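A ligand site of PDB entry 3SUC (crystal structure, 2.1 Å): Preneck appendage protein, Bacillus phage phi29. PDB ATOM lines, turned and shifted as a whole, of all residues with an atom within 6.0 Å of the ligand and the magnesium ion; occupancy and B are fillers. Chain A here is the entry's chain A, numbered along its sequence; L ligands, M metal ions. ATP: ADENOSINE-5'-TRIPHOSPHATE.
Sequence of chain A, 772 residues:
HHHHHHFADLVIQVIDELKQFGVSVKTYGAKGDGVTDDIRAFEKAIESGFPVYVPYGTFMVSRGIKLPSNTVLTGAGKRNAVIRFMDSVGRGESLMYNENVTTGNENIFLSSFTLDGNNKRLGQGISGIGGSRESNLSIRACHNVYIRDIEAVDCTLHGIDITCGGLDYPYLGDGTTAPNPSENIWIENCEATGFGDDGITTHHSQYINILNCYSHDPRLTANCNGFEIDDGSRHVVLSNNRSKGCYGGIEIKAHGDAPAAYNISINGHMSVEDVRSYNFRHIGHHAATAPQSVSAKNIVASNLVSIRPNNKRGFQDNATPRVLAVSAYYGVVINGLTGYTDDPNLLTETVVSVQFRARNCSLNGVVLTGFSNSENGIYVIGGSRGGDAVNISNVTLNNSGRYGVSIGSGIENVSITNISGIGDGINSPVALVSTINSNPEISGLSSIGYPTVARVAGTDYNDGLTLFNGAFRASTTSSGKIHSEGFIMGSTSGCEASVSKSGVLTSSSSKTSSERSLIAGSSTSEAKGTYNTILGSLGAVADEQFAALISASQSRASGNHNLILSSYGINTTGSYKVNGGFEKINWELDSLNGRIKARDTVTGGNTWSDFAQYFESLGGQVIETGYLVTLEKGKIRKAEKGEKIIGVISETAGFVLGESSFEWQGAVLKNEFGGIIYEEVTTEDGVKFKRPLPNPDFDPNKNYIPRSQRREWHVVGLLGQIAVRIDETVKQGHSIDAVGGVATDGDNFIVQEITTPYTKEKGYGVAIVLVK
O2B of the ligand lies close to OE1 of Gln 665 (3.0 Å).
An oxygen (O2B) of the ligand sits at hydrogen-bond distance from the indole nitrogen (NE1) of Trp 664, 2.8 Å away.
The guanidinium group (NE) of Arg 707 is in salt-bridge range of an oxygen (O1G) of the ligand (2.9 Å).
N of Ile 705 sits at hydrogen-bond distance from O3' of the ligand.
The guanidinium group (NH2) of Arg 710 is in salt-bridge range of an oxygen (O1G) of the ligand (2.8 Å).
An oxygen (O3G) of the ligand sits at hydrogen-bond distance from the indole nitrogen (NE1) of Trp 713, at 2.8 Å.
N1 of the ligand is in hydrogen-bond range of N of Asp 699, 3.0 Å away.
The backbone carbonyl oxygen (O) of Asp 697 is in hydrogen-bond range of a nitrogen (N6) of the ligand (3.3 Å).
An oxygen (O2') of the ligand is in hydrogen-bond range of the backbone carbonyl oxygen of Asn 703 (2.7 Å).
The guanidinium group of Arg 710 is in salt-bridge range of the side-chain carboxylate of Glu 712, at 3.1 Å.
NE of Arg 710 sits at hydrogen-bond distance from O of Pro 706, 3.2 Å away.
OH of Tyr 704 is in hydrogen-bond range of O of Ser 660.
NE of Arg 710 lies within hydrogen-bond range of O of Ile 705 (2.7 Å).
CD2 of Phe 698 touches C2 of the ligand, at 3.7 Å.
Lys 702 touches the ligand (CE to C5, 3.5 Å).
Tyr 704 touches the ligand.
Hydrophobic or aromatic side chains that line the ligand: Trp 664, Phe 698, Tyr 704, Ile 705 and Trp 713.
Of the 18 residues printed, 12 come within 4 Å of the ligand.
The nearest printed residue that does not touch the ligand is Glu 712 (4.4 Å).
No residue comes within 4 Å of the magnesium ion.
The magnesium ion is bound by an oxygen (O1A) of the ligand, 2.1 Å away.
The magnesium ion is bound by O1B of the ligand (2.4 Å).
The magnesium ion has two donor atoms within binding distance.
Slightly farther from the magnesium ion lies an oxygen (O3G) of the ligand (2.7 Å).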
ATOM      1  N   GLU A 616     -10.888   8.121  29.544  1.00  0.00           N
ATOM      2  CA  GLU A 616     -11.379   9.486  29.450  1.00  0.00           C
ATOM      3  C   GLU A 616     -12.726   9.606  30.136  1.00  0.00           C
ATOM      4  O   GLU A 616     -13.599   8.751  29.959  1.00  0.00           O
ATOM      5  CB  GLU A 616     -11.486   9.910  27.991  1.00  0.00           C
ATOM      6  CG  GLU A 616     -11.659  11.413  27.780  1.00  0.00           C
ATOM      7  CD  GLU A 616     -11.859  11.794  26.317  1.00  0.00           C
ATOM      8  OE1 GLU A 616     -12.376  12.905  26.065  1.00  0.00           O
ATOM      9  OE2 GLU A 616     -11.500  10.996  25.426  1.00  0.00           O
ATOM     10  N   SER A 660       0.407   8.186  25.918  1.00  0.00           N
ATOM     11  CA  SER A 660       0.825   9.105  24.843  1.00  0.00           C
ATOM     12  C   SER A 660       1.852  10.130  25.381  1.00  0.00           C
ATOM     13  O   SER A 660       1.711  11.337  25.181  1.00  0.00           O
ATOM     14  CB  SER A 660      -0.375   9.786  24.164  1.00  0.00           C
ATOM     15  OG  SER A 660      -1.109   8.855  23.388  1.00  0.00           O
ATOM     16  N   TRP A 664       1.455  13.367  20.357  1.00  0.00           N
ATOM     17  CA  TRP A 664       0.000  13.313  20.237  1.00  0.00           C
ATOM     18  C   TRP A 664      -0.376  11.932  19.694  1.00  0.00           C
ATOM     19  O   TRP A 664       0.334  11.364  18.859  1.00  0.00           O
ATOM     20  CB  TRP A 664      -0.529  14.448  19.344  1.00  0.00           C
ATOM     21  CG  TRP A 664      -1.952  14.278  18.868  1.00  0.00           C
ATOM     22  CD1 TRP A 664      -3.071  14.143  19.653  1.00  0.00           C
ATOM     23  CD2 TRP A 664      -2.416  14.219  17.511  1.00  0.00           C
ATOM     24  NE1 TRP A 664      -4.186  14.005  18.867  1.00  0.00           N
ATOM     25  CE2 TRP A 664      -3.813  14.044  17.557  1.00  0.00           C
ATOM     26  CE3 TRP A 664      -1.775  14.307  16.271  1.00  0.00           C
ATOM     27  CZ2 TRP A 664      -4.593  13.949  16.387  1.00  0.00           C
ATOM     28  CZ3 TRP A 664      -2.546  14.217  15.109  1.00  0.00           C
ATOM     29  CH2 TRP A 664      -3.945  14.034  15.178  1.00  0.00           C
ATOM     30  N   GLN A 665      -1.493  11.398  20.186  1.00  0.00           N
ATOM     31  CA  GLN A 665      -1.929  10.038  19.859  1.00  0.00           C
ATOM     32  C   GLN A 665      -2.179   9.786  18.364  1.00  0.00           C
ATOM     33  O   GLN A 665      -1.928   8.684  17.865  1.00  0.00           O
ATOM     34  CB  GLN A 665      -3.128   9.633  20.720  1.00  0.00           C
ATOM     35  CG  GLN A 665      -4.406  10.449  20.499  1.00  0.00           C
ATOM     36  CD  GLN A 665      -5.333   9.828  19.455  1.00  0.00           C
ATOM     37  OE1 GLN A 665      -6.018  10.548  18.717  1.00  0.00           O
ATOM     38  NE2 GLN A 665      -5.371   8.501  19.398  1.00  0.00           N
ATOM     39  N   GLY A 666      -2.654  10.824  17.662  1.00  0.00           N
ATOM     40  CA  GLY A 666      -2.986  10.693  16.249  1.00  0.00           C
ATOM     41  C   GLY A 666      -1.868  11.066  15.290  1.00  0.00           C
ATOM     42  O   GLY A 666      -2.110  11.216  14.085  1.00  0.00           O
ATOM     43  N   ASP A 697      -2.925  14.685   8.951  1.00  0.00           N
ATOM     44  CA  ASP A 697      -3.718  15.595   9.791  1.00  0.00           C
ATOM     45  C   ASP A 697      -2.933  16.145  10.985  1.00  0.00           C
ATOM     46  O   ASP A 697      -3.399  17.058  11.675  1.00  0.00           O
ATOM     47  CB  ASP A 697      -4.996  14.896  10.280  1.00  0.00           C
ATOM     48  CG  ASP A 697      -5.810  14.310   9.148  1.00  0.00           C
ATOM     49  OD1 ASP A 697      -5.468  13.210   8.672  1.00  0.00           O
ATOM     50  OD2 ASP A 697      -6.810  14.944   8.740  1.00  0.00           O
ATOM     51  N   PHE A 698      -1.753  15.588  11.228  1.00  0.00           N
ATOM     52  CA  PHE A 698      -0.863  16.052  12.299  1.00  0.00           C
ATOM     53  C   PHE A 698      -0.366  17.469  12.044  1.00  0.00           C
ATOM     54  O   PHE A 698       0.084  17.793  10.932  1.00  0.00           O
ATOM     55  CB  PHE A 698       0.312  15.081  12.489  1.00  0.00           C
ATOM     56  CG  PHE A 698       1.416  15.612  13.375  1.00  0.00           C
ATOM     57  CD1 PHE A 698       2.603  16.089  12.818  1.00  0.00           C
ATOM     58  CD2 PHE A 698       1.274  15.628  14.758  1.00  0.00           C
ATOM     59  CE1 PHE A 698       3.633  16.583  13.625  1.00  0.00           C
ATOM     60  CE2 PHE A 698       2.288  16.117  15.587  1.00  0.00           C
ATOM     61  CZ  PHE A 698       3.473  16.592  15.021  1.00  0.00           C
ATOM     62  N   ASP A 699      -0.458  18.316  13.068  1.00  0.00           N
ATOM     63  CA  ASP A 699       0.014  19.688  12.999  1.00  0.00           C
ATOM     64  C   ASP A 699       1.153  19.909  14.001  1.00  0.00           C
ATOM     65  O   ASP A 699       0.915  19.971  15.207  1.00  0.00           O
ATOM     66  CB  ASP A 699      -1.153  20.664  13.249  1.00  0.00           C
ATOM     67  CG  ASP A 699      -0.734  22.134  13.122  1.00  0.00           C
ATOM     68  OD1 ASP A 699      -1.385  22.978  13.780  1.00  0.00           O
ATOM     69  OD2 ASP A 699       0.221  22.437  12.385  1.00  0.00           O
ATOM     70  N   PRO A 700       2.393  20.029  13.497  1.00  0.00           N
ATOM     71  CA  PRO A 700       3.584  20.246  14.341  1.00  0.00           C
ATOM     72  C   PRO A 700       3.609  21.621  15.015  1.00  0.00           C
ATOM     73  O   PRO A 700       4.444  21.859  15.904  1.00  0.00           O
ATOM     74  CB  PRO A 700       4.743  20.108  13.356  1.00  0.00           C
ATOM     75  CG  PRO A 700       4.165  20.447  12.024  1.00  0.00           C
ATOM     76  CD  PRO A 700       2.749  19.958  12.058  1.00  0.00           C
ATOM     77  N   LYS A 702       0.814  22.881  16.656  1.00  0.00           N
ATOM     78  CA  LYS A 702       0.074  22.612  17.891  1.00  0.00           C
ATOM     79  C   LYS A 702       0.988  22.099  18.998  1.00  0.00           C
ATOM     80  O   LYS A 702       1.680  21.086  18.846  1.00  0.00           O
ATOM     81  CB  LYS A 702      -1.075  21.627  17.642  1.00  0.00           C
ATOM     82  CG  LYS A 702      -2.225  22.217  16.824  1.00  0.00           C
ATOM     83  CD  LYS A 702      -3.288  21.180  16.497  1.00  0.00           C
ATOM     84  CE  LYS A 702      -4.362  21.087  17.588  1.00  0.00           C
ATOM     85  NZ  LYS A 702      -5.311  22.237  17.556  1.00  0.00           N
ATOM     86  N   ASN A 703       1.014  22.837  20.108  1.00  0.00           N
ATOM     87  CA  ASN A 703       1.867  22.522  21.238  1.00  0.00           C
ATOM     88  C   ASN A 703       1.259  21.377  22.049  1.00  0.00           C
ATOM     89  O   ASN A 703       0.205  21.534  22.673  1.00  0.00           O
ATOM     90  CB  ASN A 703       2.066  23.760  22.124  1.00  0.00           C
ATOM     91  CG  ASN A 703       3.352  23.710  22.916  1.00  0.00           C
ATOM     92  OD1 ASN A 703       3.519  22.876  23.813  1.00  0.00           O
ATOM     93  ND2 ASN A 703       4.272  24.623  22.614  1.00  0.00           N
ATOM     94  N   TYR A 704       1.916  20.213  22.014  1.00  0.00           N
ATOM     95  CA  TYR A 704       1.372  18.996  22.629  1.00  0.00           C
ATOM     96  C   TYR A 704       1.379  19.008  24.166  1.00  0.00           C
ATOM     97  O   TYR A 704       2.424  19.197  24.802  1.00  0.00           O
ATOM     98  CB  TYR A 704       2.062  17.735  22.100  1.00  0.00           C
ATOM     99  CG  TYR A 704       1.469  16.468  22.689  1.00  0.00           C
ATOM    100  CD1 TYR A 704       2.264  15.557  23.389  1.00  0.00           C
ATOM    101  CD2 TYR A 704       0.100  16.185  22.561  1.00  0.00           C
ATOM    102  CE1 TYR A 704       1.709  14.390  23.943  1.00  0.00           C
ATOM    103  CE2 TYR A 704      -0.454  15.040  23.110  1.00  0.00           C
ATOM    104  CZ  TYR A 704       0.354  14.142  23.786  1.00  0.00           C
ATOM    105  OH  TYR A 704      -0.218  13.009  24.323  1.00  0.00           O
ATOM    106  N   ILE A 705       0.196  18.802  24.725  1.00  0.00           N
ATOM    107  CA  ILE A 705       0.028  18.567  26.154  1.00  0.00           C
ATOM    108  C   ILE A 705      -0.445  17.114  26.333  1.00  0.00           C
ATOM    109  O   ILE A 705      -1.503  16.748  25.808  1.00  0.00           O
ATOM    110  CB  ILE A 705      -0.976  19.558  26.808  1.00  0.00           C
ATOM    111  CG1 ILE A 705      -0.540  21.013  26.550  1.00  0.00           C
ATOM    112  CG2 ILE A 705      -1.100  19.301  28.311  1.00  0.00           C
ATOM    113  CD1 ILE A 705      -1.675  22.030  26.573  1.00  0.00           C
ATOM    114  N   PRO A 706       0.346  16.291  27.035  1.00  0.00           N
ATOM    115  CA  PRO A 706       0.062  14.857  27.204  1.00  0.00           C
ATOM    116  C   PRO A 706      -1.151  14.575  28.101  1.00  0.00           C
ATOM    117  O   PRO A 706      -1.530  15.418  28.922  1.00  0.00           O
ATOM    118  CB  PRO A 706       1.344  14.295  27.831  1.00  0.00           C
ATOM    119  CG  PRO A 706       2.369  15.388  27.697  1.00  0.00           C
ATOM    120  CD  PRO A 706       1.604  16.666  27.716  1.00  0.00           C
ATOM    121  N   ARG A 707      -1.734  13.388  27.932  1.00  0.00           N
ATOM    122  CA  ARG A 707      -2.901  12.944  28.686  1.00  0.00           C
ATOM    123  C   ARG A 707      -2.673  12.999  30.195  1.00  0.00           C
ATOM    124  O   ARG A 707      -3.599  13.254  30.973  1.00  0.00           O
ATOM    125  CB  ARG A 707      -3.282  11.528  28.274  1.00  0.00           C
ATOM    126  CG  ARG A 707      -3.807  11.407  26.854  1.00  0.00           C
ATOM    127  CD  ARG A 707      -3.914   9.958  26.418  1.00  0.00           C
ATOM    128  NE  ARG A 707      -4.700   9.806  25.199  1.00  0.00           N
ATOM    129  CZ  ARG A 707      -4.892   8.651  24.562  1.00  0.00           C
ATOM    130  NH1 ARG A 707      -4.335   7.527  25.009  1.00  0.00           N
ATOM    131  NH2 ARG A 707      -5.634   8.619  23.458  1.00  0.00           N
ATOM    132  N   ARG A 710      -3.645  16.421  31.160  1.00  0.00           N
ATOM    133  CA  ARG A 710      -5.051  16.761  30.920  1.00  0.00           C
ATOM    134  C   ARG A 710      -5.984  16.338  32.051  1.00  0.00           C
ATOM    135  O   ARG A 710      -5.710  15.366  32.774  1.00  0.00           O
ATOM    136  CB  ARG A 710      -5.546  16.178  29.597  1.00  0.00           C
ATOM    137  CG  ARG A 710      -5.643  17.194  28.471  1.00  0.00           C
ATOM    138  CD  ARG A 710      -4.319  17.392  27.749  1.00  0.00           C
ATOM    139  NE  ARG A 710      -3.876  16.235  26.949  1.00  0.00           N
ATOM    140  CZ  ARG A 710      -4.660  15.475  26.191  1.00  0.00           C
ATOM    141  NH1 ARG A 710      -5.962  15.707  26.079  1.00  0.00           N
ATOM    142  NH2 ARG A 710      -4.115  14.468  25.525  1.00  0.00           N
ATOM    143  N   GLU A 712      -9.372  15.449  31.813  1.00  0.00           N
ATOM    144  CA  GLU A 712     -10.375  14.428  31.488  1.00  0.00           C
ATOM    145  C   GLU A 712      -9.816  13.004  31.446  1.00  0.00           C
ATOM    146  O   GLU A 712     -10.570  12.028  31.523  1.00  0.00           O
ATOM    147  CB  GLU A 712     -11.095  14.794  30.172  1.00  0.00           C
ATOM    148  CG  GLU A 712     -10.265  14.659  28.884  1.00  0.00           C
ATOM    149  CD  GLU A 712      -9.318  15.825  28.617  1.00  0.00           C
ATOM    150  OE1 GLU A 712      -9.190  16.734  29.477  1.00  0.00           O
ATOM    151  OE2 GLU A 712      -8.688  15.825  27.541  1.00  0.00           O
ATOM    152  N   TRP A 713      -8.491  12.890  31.346  1.00  0.00           N
ATOM    153  CA  TRP A 713      -7.834  11.586  31.280  1.00  0.00           C
ATOM    154  C   TRP A 713      -7.401  11.061  32.643  1.00  0.00           C
ATOM    155  O   TRP A 713      -6.677  11.724  33.386  1.00  0.00           O
ATOM    156  CB  TRP A 713      -6.651  11.629  30.314  1.00  0.00           C
ATOM    157  CG  TRP A 713      -7.105  11.675  28.893  1.00  0.00           C
ATOM    158  CD1 TRP A 713      -7.281  12.787  28.132  1.00  0.00           C
ATOM    159  CD2 TRP A 713      -7.457  10.556  28.066  1.00  0.00           C
ATOM    160  NE1 TRP A 713      -7.720  12.433  26.878  1.00  0.00           N
ATOM    161  CE2 TRP A 713      -7.833  11.071  26.814  1.00  0.00           C
ATOM    162  CE3 TRP A 713      -7.481   9.171  28.266  1.00  0.00           C
ATOM    163  CZ2 TRP A 713      -8.245  10.250  25.752  1.00  0.00           C
ATOM    164  CZ3 TRP A 713      -7.891   8.355  27.224  1.00  0.00           C
ATOM    165  CH2 TRP A 713      -8.266   8.894  25.977  1.00  0.00           C
HETATM  166  PG  ATP L   1      -6.082  12.623  23.372  1.00  0.00           P
HETATM  167  O1G ATP L   1      -4.648  12.360  23.778  1.00  0.00           O
HETATM  168  O2G ATP L   1      -6.788  11.426  22.785  1.00  0.00           O
HETATM  169  O3G ATP L   1      -6.890  13.372  24.412  1.00  0.00           O
HETATM  170  PB  ATP L   1      -7.089  13.962  21.066  1.00  0.00           P
HETATM  171  O1B ATP L   1      -8.442  13.724  21.707  1.00  0.00           O
HETATM  172  O2B ATP L   1      -6.726  13.210  19.805  1.00  0.00           O
HETATM  173  O3B ATP L   1      -5.936  13.681  22.165  1.00  0.00           O
HETATM  174  PA  ATP L   1      -6.991  16.692  21.871  1.00  0.00           P
HETATM  175  O1A ATP L   1      -7.962  16.290  22.969  1.00  0.00           O
HETATM  176  O2A ATP L   1      -7.160  18.021  21.185  1.00  0.00           O
HETATM  177  O3A ATP L   1      -6.952  15.544  20.742  1.00  0.00           O
HETATM  178  O5' ATP L   1      -5.495  16.618  22.477  1.00  0.00           O
HETATM  179  C5' ATP L   1      -4.963  17.654  23.308  1.00  0.00           C
HETATM  180  C4' ATP L   1      -3.498  17.908  22.963  1.00  0.00           C
HETATM  181  O4' ATP L   1      -3.110  17.203  21.772  1.00  0.00           O
HETATM  182  C3' ATP L   1      -3.258  19.385  22.715  1.00  0.00           C
HETATM  183  O3' ATP L   1      -2.270  19.867  23.631  1.00  0.00           O
HETATM  184  C2' ATP L   1      -2.800  19.506  21.267  1.00  0.00           C
HETATM  185  O2' ATP L   1      -1.588  20.253  21.153  1.00  0.00           O
HETATM  186  C1' ATP L   1      -2.572  18.081  20.779  1.00  0.00           C
HETATM  187  N9  ATP L   1      -3.255  17.883  19.470  1.00  0.00           N
HETATM  188  C8  ATP L   1      -4.581  17.732  19.279  1.00  0.00           C
HETATM  189  N7  ATP L   1      -4.885  17.578  17.971  1.00  0.00           N
HETATM  190  C5  ATP L   1      -3.727  17.637  17.282  1.00  0.00           C
HETATM  191  C6  ATP L   1      -3.327  17.544  15.854  1.00  0.00           C
HETATM  192  N6  ATP L   1      -4.255  17.359  14.880  1.00  0.00           N
HETATM  193  N1  ATP L   1      -2.010  17.647  15.553  1.00  0.00           N
HETATM  194  C2  ATP L   1      -1.082  17.830  16.518  1.00  0.00           C
HETATM  195  N3  ATP L   1      -1.369  17.922  17.834  1.00  0.00           N
HETATM  196  C4  ATP L   1      -2.658  17.835  18.273  1.00  0.00           C
HETATM  197 MG    MG M   1      -9.174  14.726  23.703  1.00  0.00          MG
